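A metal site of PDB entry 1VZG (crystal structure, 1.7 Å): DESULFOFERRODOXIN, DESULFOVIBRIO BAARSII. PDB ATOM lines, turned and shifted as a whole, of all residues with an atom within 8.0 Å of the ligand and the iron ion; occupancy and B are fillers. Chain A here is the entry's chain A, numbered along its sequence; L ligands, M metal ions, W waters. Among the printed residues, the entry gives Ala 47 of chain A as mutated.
The side-chain amino group (NZ) of Lys 48 lies within hydrogen-bond range of a nitrogen (N2) of the ligand (3.1 Å).
The backbone NH (N) of Ala 45 is in hydrogen-bond range of a nitrogen (N5) of the ligand.
The iron ion is bound by a ring nitrogen (ND1) of His 119 (2.1 Å), a ring nitrogen (NE2) of His 69 (2.2 Å), a ring nitrogen (NE2) of His 75 (2.2 Å), a ring nitrogen (NE2) of His 49 (2.3 Å), a nitrogen (N1) of the ligand (2.4 Å) and the side-chain sulfur of Cys 116 (2.6 Å).
The iron ion has six donor atoms within binding distance.
The backbone carbonyl oxygen of Val 64 lies within hydrogen-bond range of the backbone NH of His 69 (2.9 Å).
SG of Cys 116 lies close to N of Ile 118, at 3.5 Å.
O of His 49 lies close to OE2 of Glu 114 (2.6 Å).
The side-chain carboxylate of Glu 114 sits at hydrogen-bond distance from the backbone NH of Cys 116.
The backbone carbonyl oxygen (O) of His 119 lies within hydrogen-bond range of the indole nitrogen (NE1) of Trp 122, 2.9 Å away.
ND1 of His 49 lies within hydrogen-bond range of O of Ala 45 (2.7 Å).
Ala 44 touches the ligand (CB to N5, 3.7 Å).
CG of Pro 70 touches N2 of the ligand, 3.6 Å away.
Hydrophobic or aromatic side chains within 4 Å of the ligand: Ala 44, Ala 45, His 49, His 69, Pro 70, His 75 and His 119.
Of the 25 residues printed, 8 come within 4 Å of the ligand.
The nearest printed residue that does not touch the ligand is Cys 116 (5.0 Å).
Water W1 bridges a ring nitrogen (NE2) of His 119 and a nitrogen (N4) of the ligand.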
ATOM      1  N   VAL A  42      -2.496 -15.662  18.399  1.00  0.00           N
ATOM      2  CA  VAL A  42      -1.576 -16.652  18.926  1.00  0.00           C
ATOM      3  C   VAL A  42      -2.228 -17.620  19.904  1.00  0.00           C
ATOM      4  O   VAL A  42      -3.067 -17.235  20.717  1.00  0.00           O
ATOM      5  CB  VAL A  42      -0.375 -15.965  19.629  1.00  0.00           C
ATOM      6  CG1 VAL A  42       0.495 -17.003  20.343  1.00  0.00           C
ATOM      7  CG2 VAL A  42       0.443 -15.186  18.613  1.00  0.00           C
ATOM      8  N   ASP A  43      -1.841 -18.889  19.810  1.00  0.00           N
ATOM      9  CA  ASP A  43      -2.371 -19.923  20.678  1.00  0.00           C
ATOM     10  C   ASP A  43      -1.681 -19.835  22.043  1.00  0.00           C
ATOM     11  O   ASP A  43      -0.735 -20.571  22.325  1.00  0.00           O
ATOM     12  CB  ASP A  43      -2.115 -21.296  20.063  1.00  0.00           C
ATOM     13  CG  ASP A  43      -2.821 -22.420  20.801  1.00  0.00           C
ATOM     14  OD1 ASP A  43      -2.570 -22.597  22.014  1.00  0.00           O
ATOM     15  OD2 ASP A  43      -3.626 -23.133  20.162  1.00  0.00           O
ATOM     16  N   ALA A  44      -2.152 -18.920  22.885  1.00  0.00           N
ATOM     17  CA  ALA A  44      -1.600 -18.735  24.225  1.00  0.00           C
ATOM     18  C   ALA A  44      -2.725 -18.416  25.204  1.00  0.00           C
ATOM     19  O   ALA A  44      -3.808 -18.000  24.793  1.00  0.00           O
ATOM     20  CB  ALA A  44      -0.551 -17.627  24.214  1.00  0.00           C
ATOM     21  N   ALA A  45      -2.457 -18.578  26.491  1.00  0.00           N
ATOM     22  CA  ALA A  45      -3.452 -18.320  27.529  1.00  0.00           C
ATOM     23  C   ALA A  45      -3.956 -16.879  27.506  1.00  0.00           C
ATOM     24  O   ALA A  45      -3.186 -15.938  27.658  1.00  0.00           O
ATOM     25  CB  ALA A  45      -2.879 -18.651  28.885  1.00  0.00           C
ATOM     26  N   LYS A  46      -5.270 -16.728  27.348  1.00  0.00           N
ATOM     27  CA  LYS A  46      -5.881 -15.403  27.319  1.00  0.00           C
ATOM     28  C   LYS A  46      -5.856 -14.772  28.706  1.00  0.00           C
ATOM     29  O   LYS A  46      -5.750 -13.550  28.832  1.00  0.00           O
ATOM     30  CB  LYS A  46      -7.323 -15.497  26.833  1.00  0.00           C
ATOM     31  CG  LYS A  46      -7.473 -16.066  25.428  1.00  0.00           C
ATOM     32  CD  LYS A  46      -8.918 -16.006  24.958  1.00  0.00           C
ATOM     33  CE  LYS A  46      -9.854 -16.709  25.948  1.00  0.00           C
ATOM     34  NZ  LYS A  46      -9.513 -18.148  26.124  1.00  0.00           N
ATOM     35  N   ALA A  47      -5.948 -15.596  29.736  1.00  0.00           N
ATOM     36  CA  ALA A  47      -5.941 -15.111  31.111  1.00  0.00           C
ATOM     37  C   ALA A  47      -4.743 -14.219  31.432  1.00  0.00           C
ATOM     38  O   ALA A  47      -4.859 -13.248  32.174  1.00  0.00           O
ATOM     39  CB  ALA A  47      -5.978 -16.294  32.084  1.00  0.00           C
ATOM     40  N   LYS A  48      -3.594 -14.558  30.862  1.00  0.00           N
ATOM     41  CA  LYS A  48      -2.392 -13.761  31.102  1.00  0.00           C
ATOM     42  C   LYS A  48      -2.034 -12.790  29.983  1.00  0.00           C
ATOM     43  O   LYS A  48      -1.179 -11.923  30.167  1.00  0.00           O
ATOM     44  CB  LYS A  48      -1.182 -14.670  31.359  1.00  0.00           C
ATOM     45  CG  LYS A  48      -1.257 -15.470  32.656  1.00  0.00           C
ATOM     46  CD  LYS A  48       0.061 -16.173  32.936  1.00  0.00           C
ATOM     47  CE  LYS A  48       0.002 -16.971  34.239  1.00  0.00           C
ATOM     48  NZ  LYS A  48       1.279 -17.682  34.480  1.00  0.00           N
ATOM     49  N   HIS A  49      -2.684 -12.924  28.827  1.00  0.00           N
ATOM     50  CA  HIS A  49      -2.371 -12.049  27.697  1.00  0.00           C
ATOM     51  C   HIS A  49      -3.389 -11.010  27.266  1.00  0.00           C
ATOM     52  O   HIS A  49      -3.022  -9.967  26.727  1.00  0.00           O
ATOM     53  CB  HIS A  49      -1.993 -12.887  26.475  1.00  0.00           C
ATOM     54  CG  HIS A  49      -0.745 -13.703  26.660  1.00  0.00           C
ATOM     55  ND1 HIS A  49      -0.775 -15.019  27.036  1.00  0.00           N
ATOM     56  CD2 HIS A  49       0.559 -13.367  26.545  1.00  0.00           C
ATOM     57  CE1 HIS A  49       0.459 -15.475  27.144  1.00  0.00           C
ATOM     58  NE2 HIS A  49       1.286 -14.492  26.858  1.00  0.00           N
ATOM     59  N   VAL A  64      -2.110  -6.624  32.428  1.00  0.00           N
ATOM     60  CA  VAL A  64      -1.934  -7.776  31.546  1.00  0.00           C
ATOM     61  C   VAL A  64      -1.608  -9.010  32.381  1.00  0.00           C
ATOM     62  O   VAL A  64      -0.478  -9.150  32.838  1.00  0.00           O
ATOM     63  CB  VAL A  64      -0.789  -7.523  30.546  1.00  0.00           C
ATOM     64  CG1 VAL A  64      -0.593  -8.741  29.653  1.00  0.00           C
ATOM     65  CG2 VAL A  64      -1.082  -6.290  29.704  1.00  0.00           C
ATOM     66  N   VAL A  67      -4.883 -12.483  34.876  1.00  0.00           N
ATOM     67  CA  VAL A  67      -3.895 -13.099  35.758  1.00  0.00           C
ATOM     68  C   VAL A  67      -2.584 -12.405  35.382  1.00  0.00           C
ATOM     69  O   VAL A  67      -2.248 -12.325  34.206  1.00  0.00           O
ATOM     70  CB  VAL A  67      -3.759 -14.609  35.495  1.00  0.00           C
ATOM     71  CG1 VAL A  67      -2.657 -15.201  36.360  1.00  0.00           C
ATOM     72  CG2 VAL A  67      -5.078 -15.309  35.772  1.00  0.00           C
ATOM     73  N   ALA A  68      -1.878 -11.892  36.380  1.00  0.00           N
ATOM     74  CA  ALA A  68      -0.608 -11.199  36.139  1.00  0.00           C
ATOM     75  C   ALA A  68       0.354 -11.982  35.253  1.00  0.00           C
ATOM     76  O   ALA A  68       0.726 -13.112  35.567  1.00  0.00           O
ATOM     77  CB  ALA A  68       0.055 -10.866  37.467  1.00  0.00           C
ATOM     78  N   HIS A  69       0.767 -11.370  34.147  1.00  0.00           N
ATOM     79  CA  HIS A  69       1.706 -12.004  33.212  1.00  0.00           C
ATOM     80  C   HIS A  69       3.132 -11.886  33.741  1.00  0.00           C
ATOM     81  O   HIS A  69       3.477 -10.912  34.405  1.00  0.00           O
ATOM     82  CB  HIS A  69       1.593 -11.335  31.830  1.00  0.00           C
ATOM     83  CG  HIS A  69       2.442 -11.979  30.769  1.00  0.00           C
ATOM     84  ND1 HIS A  69       3.807 -11.814  30.705  1.00  0.00           N
ATOM     85  CD2 HIS A  69       2.110 -12.789  29.736  1.00  0.00           C
ATOM     86  CE1 HIS A  69       4.280 -12.492  29.674  1.00  0.00           C
ATOM     87  NE2 HIS A  69       3.271 -13.096  29.072  1.00  0.00           N
ATOM     88  N   PRO A  70       3.970 -12.892  33.464  1.00  0.00           N
ATOM     89  CA  PRO A  70       5.354 -12.859  33.933  1.00  0.00           C
ATOM     90  C   PRO A  70       6.134 -11.670  33.376  1.00  0.00           C
ATOM     91  O   PRO A  70       5.856 -11.190  32.273  1.00  0.00           O
ATOM     92  CB  PRO A  70       5.929 -14.182  33.432  1.00  0.00           C
ATOM     93  CG  PRO A  70       4.739 -15.083  33.425  1.00  0.00           C
ATOM     94  CD  PRO A  70       3.659 -14.196  32.849  1.00  0.00           C
ATOM     95  N   GLU A  72       9.772 -11.591  33.286  1.00  0.00           N
ATOM     96  CA  GLU A  72      11.099 -12.167  33.411  1.00  0.00           C
ATOM     97  C   GLU A  72      11.976 -11.745  32.236  1.00  0.00           C
ATOM     98  O   GLU A  72      11.473 -11.375  31.185  1.00  0.00           O
ATOM     99  CB  GLU A  72      11.007 -13.703  33.442  1.00  0.00           C
ATOM    100  CG  GLU A  72      10.092 -14.253  34.519  1.00  0.00           C
ATOM    101  CD  GLU A  72      10.078 -15.771  34.535  1.00  0.00           C
ATOM    102  OE1 GLU A  72      11.167 -16.367  34.694  1.00  0.00           O
ATOM    103  OE2 GLU A  72       8.987 -16.368  34.396  1.00  0.00           O
ATOM    104  N   HIS A  75      10.906 -13.605  29.213  1.00  0.00           N
ATOM    105  CA  HIS A  75       9.473 -13.684  28.947  1.00  0.00           C
ATOM    106  C   HIS A  75       8.778 -12.564  29.690  1.00  0.00           C
ATOM    107  O   HIS A  75       8.549 -12.652  30.897  1.00  0.00           O
ATOM    108  CB  HIS A  75       8.929 -15.035  29.419  1.00  0.00           C
ATOM    109  CG  HIS A  75       7.478 -15.216  29.151  1.00  0.00           C
ATOM    110  ND1 HIS A  75       6.696 -16.125  29.840  1.00  0.00           N
ATOM    111  CD2 HIS A  75       6.646 -14.616  28.266  1.00  0.00           C
ATOM    112  CE1 HIS A  75       5.459 -16.070  29.389  1.00  0.00           C
ATOM    113  NE2 HIS A  75       5.397 -15.157  28.435  1.00  0.00           N
ATOM    114  N   TYR A  76       8.423 -11.501  28.971  1.00  0.00           N
ATOM    115  CA  TYR A  76       7.773 -10.369  29.598  1.00  0.00           C
ATOM    116  C   TYR A  76       6.950  -9.575  28.598  1.00  0.00           C
ATOM    117  O   TYR A  76       6.989  -9.830  27.401  1.00  0.00           O
ATOM    118  CB  TYR A  76       8.824  -9.431  30.210  1.00  0.00           C
ATOM    119  CG  TYR A  76       9.764  -8.795  29.205  1.00  0.00           C
ATOM    120  CD1 TYR A  76      10.710  -9.552  28.519  1.00  0.00           C
ATOM    121  CD2 TYR A  76       9.704  -7.428  28.937  1.00  0.00           C
ATOM    122  CE1 TYR A  76      11.572  -8.966  27.588  1.00  0.00           C
ATOM    123  CE2 TYR A  76      10.566  -6.824  28.020  1.00  0.00           C
ATOM    124  CZ  TYR A  76      11.496  -7.607  27.351  1.00  0.00           C
ATOM    125  OH  TYR A  76      12.357  -7.017  26.437  1.00  0.00           O
ATOM    126  N   ILE A  77       6.201  -8.608  29.118  1.00  0.00           N
ATOM    127  CA  ILE A  77       5.375  -7.729  28.289  1.00  0.00           C
ATOM    128  C   ILE A  77       6.289  -6.567  27.932  1.00  0.00           C
ATOM    129  O   ILE A  77       6.755  -5.837  28.821  1.00  0.00           O
ATOM    130  CB  ILE A  77       4.141  -7.211  29.070  1.00  0.00           C
ATOM    131  CG1 ILE A  77       3.349  -8.406  29.628  1.00  0.00           C
ATOM    132  CG2 ILE A  77       3.253  -6.356  28.158  1.00  0.00           C
ATOM    133  CD1 ILE A  77       2.918  -9.406  28.581  1.00  0.00           C
ATOM    134  N   GLU A 114      -1.133  -5.025  24.099  1.00  0.00           N
ATOM    135  CA  GLU A 114       0.089  -5.397  24.808  1.00  0.00           C
ATOM    136  C   GLU A 114       0.833  -6.371  23.930  1.00  0.00           C
ATOM    137  O   GLU A 114       0.220  -7.132  23.171  1.00  0.00           O
ATOM    138  CB  GLU A 114      -0.247  -6.054  26.159  1.00  0.00           C
ATOM    139  CG  GLU A 114      -0.950  -7.409  26.066  1.00  0.00           C
ATOM    140  CD  GLU A 114       0.009  -8.590  26.001  1.00  0.00           C
ATOM    141  OE1 GLU A 114       1.235  -8.380  25.869  1.00  0.00           O
ATOM    142  OE2 GLU A 114      -0.485  -9.743  26.097  1.00  0.00           O
ATOM    143  N   TYR A 115       2.152  -6.330  24.003  1.00  0.00           N
ATOM    144  CA  TYR A 115       2.967  -7.237  23.212  1.00  0.00           C
ATOM    145  C   TYR A 115       3.892  -8.043  24.114  1.00  0.00           C
ATOM    146  O   TYR A 115       4.663  -7.474  24.895  1.00  0.00           O
ATOM    147  CB  TYR A 115       3.789  -6.470  22.169  1.00  0.00           C
ATOM    148  CG  TYR A 115       4.579  -7.373  21.253  1.00  0.00           C
ATOM    149  CD1 TYR A 115       5.874  -7.778  21.580  1.00  0.00           C
ATOM    150  CD2 TYR A 115       4.012  -7.864  20.080  1.00  0.00           C
ATOM    151  CE1 TYR A 115       6.595  -8.642  20.751  1.00  0.00           C
ATOM    152  CE2 TYR A 115       4.717  -8.728  19.246  1.00  0.00           C
ATOM    153  CZ  TYR A 115       6.004  -9.115  19.593  1.00  0.00           C
ATOM    154  OH  TYR A 115       6.701  -9.989  18.784  1.00  0.00           O
ATOM    155  N   CYS A 116       3.781  -9.363  24.037  1.00  0.00           N
ATOM    156  CA  CYS A 116       4.607 -10.283  24.804  1.00  0.00           C
ATOM    157  C   CYS A 116       5.730 -10.765  23.874  1.00  0.00           C
ATOM    158  O   CYS A 116       5.466 -11.204  22.756  1.00  0.00           O
ATOM    159  CB  CYS A 116       3.774 -11.465  25.283  1.00  0.00           C
ATOM    160  SG  CYS A 116       4.728 -12.799  26.073  1.00  0.00           S
ATOM    161  N   ASN A 117       6.976 -10.687  24.346  1.00  0.00           N
ATOM    162  CA  ASN A 117       8.100 -11.079  23.505  1.00  0.00           C
ATOM    163  C   ASN A 117       7.989 -12.505  22.972  1.00  0.00           C
ATOM    164  O   ASN A 117       8.546 -12.828  21.917  1.00  0.00           O
ATOM    165  CB  ASN A 117       9.432 -10.905  24.275  1.00  0.00           C
ATOM    166  CG  ASN A 117       9.621 -11.943  25.366  1.00  0.00           C
ATOM    167  OD1 ASN A 117       8.729 -12.178  26.180  1.00  0.00           O
ATOM    168  ND2 ASN A 117      10.796 -12.560  25.388  1.00  0.00           N
ATOM    169  N   ILE A 118       7.264 -13.350  23.696  1.00  0.00           N
ATOM    170  CA  ILE A 118       7.099 -14.732  23.272  1.00  0.00           C
ATOM    171  C   ILE A 118       5.742 -15.024  22.631  1.00  0.00           C
ATOM    172  O   ILE A 118       5.672 -15.665  21.588  1.00  0.00           O
ATOM    173  CB  ILE A 118       7.280 -15.706  24.462  1.00  0.00           C
ATOM    174  CG1 ILE A 118       8.697 -15.581  25.030  1.00  0.00           C
ATOM    175  CG2 ILE A 118       7.009 -17.149  24.021  1.00  0.00           C
ATOM    176  CD1 ILE A 118       9.782 -15.835  24.014  1.00  0.00           C
ATOM    177  N   HIS A 119       4.672 -14.526  23.245  1.00  0.00           N
ATOM    178  CA  HIS A 119       3.331 -14.817  22.751  1.00  0.00           C
ATOM    179  C   HIS A 119       2.607 -13.813  21.868  1.00  0.00           C
ATOM    180  O   HIS A 119       1.398 -13.900  21.681  1.00  0.00           O
ATOM    181  CB  HIS A 119       2.442 -15.201  23.936  1.00  0.00           C
ATOM    182  CG  HIS A 119       3.018 -16.318  24.754  1.00  0.00           C
ATOM    183  ND1 HIS A 119       3.529 -16.119  26.015  1.00  0.00           N
ATOM    184  CD2 HIS A 119       3.221 -17.619  24.455  1.00  0.00           C
ATOM    185  CE1 HIS A 119       4.035 -17.261  26.455  1.00  0.00           C
ATOM    186  NE2 HIS A 119       3.862 -18.187  25.534  1.00  0.00           N
ATOM    187  N   GLY A 120       3.341 -12.842  21.343  1.00  0.00           N
ATOM    188  CA  GLY A 120       2.743 -11.879  20.439  1.00  0.00           C
ATOM    189  C   GLY A 120       1.898 -10.717  20.919  1.00  0.00           C
ATOM    190  O   GLY A 120       1.950 -10.285  22.069  1.00  0.00           O
ATOM    191  N   TRP A 122      -1.713  -8.689  21.559  1.00  0.00           N
ATOM    192  CA  TRP A 122      -3.054  -8.901  22.110  1.00  0.00           C
ATOM    193  C   TRP A 122      -3.776  -7.586  22.348  1.00  0.00           C
ATOM    194  O   TRP A 122      -3.140  -6.558  22.606  1.00  0.00           O
ATOM    195  CB  TRP A 122      -2.982  -9.671  23.418  1.00  0.00           C
ATOM    196  CG  TRP A 122      -2.395 -11.019  23.257  1.00  0.00           C
ATOM    197  CD1 TRP A 122      -1.083 -11.321  23.093  1.00  0.00           C
ATOM    198  CD2 TRP A 122      -3.118 -12.245  23.198  1.00  0.00           C
ATOM    199  NE1 TRP A 122      -0.937 -12.681  22.935  1.00  0.00           N
ATOM    200  CE2 TRP A 122      -2.170 -13.273  22.996  1.00  0.00           C
ATOM    201  CE3 TRP A 122      -4.476 -12.592  23.292  1.00  0.00           C
ATOM    202  CZ2 TRP A 122      -2.531 -14.620  22.883  1.00  0.00           C
ATOM    203  CZ3 TRP A 122      -4.833 -13.930  23.184  1.00  0.00           C
ATOM    204  CH2 TRP A 122      -3.868 -14.930  22.982  1.00  0.00           C
HETATM  205  N1  LIG L   1       2.496 -15.976  29.179  1.00  0.00           N
HETATM  206  C1  LIG L   1       2.329 -17.095  29.456  1.00  0.00           C
HETATM  207 FE1  LIG L   1       2.043 -18.956  29.912  1.00  0.00          FE
HETATM  208  C2  LIG L   1       3.024 -18.605  31.554  1.00  0.00           C
HETATM  209  N2  LIG L   1       3.609 -18.392  32.529  1.00  0.00           N
HETATM  210  C3  LIG L   1       0.312 -18.792  30.599  1.00  0.00           C
HETATM  211  N3  LIG L   1      -0.769 -18.690  31.033  1.00  0.00           N
HETATM  212  C4  LIG L   1       3.763 -19.285  29.122  1.00  0.00           C
HETATM  213  N4  LIG L   1       4.795 -19.483  28.636  1.00  0.00           N
HETATM  214  C5  LIG L   1       1.196 -19.280  28.229  1.00  0.00           C
HETATM  215  N5  LIG L   1       0.684 -19.476  27.197  1.00  0.00           N
HETATM  216  C6  LIG L   1       1.903 -20.821  30.350  1.00  0.00           C
HETATM  217  N6  LIG L   1       1.813 -21.950  30.618  1.00  0.00           N
HETATM  218 FE    FE M   1       3.441 -14.610  27.497  1.00  0.00          FE
HETATM  219  O   HOH W   1       4.745 -20.948  25.497  1.00  0.00           O
HETATM  220  O   HOH W   2      -3.237 -18.915  32.559  1.00  0.00           O
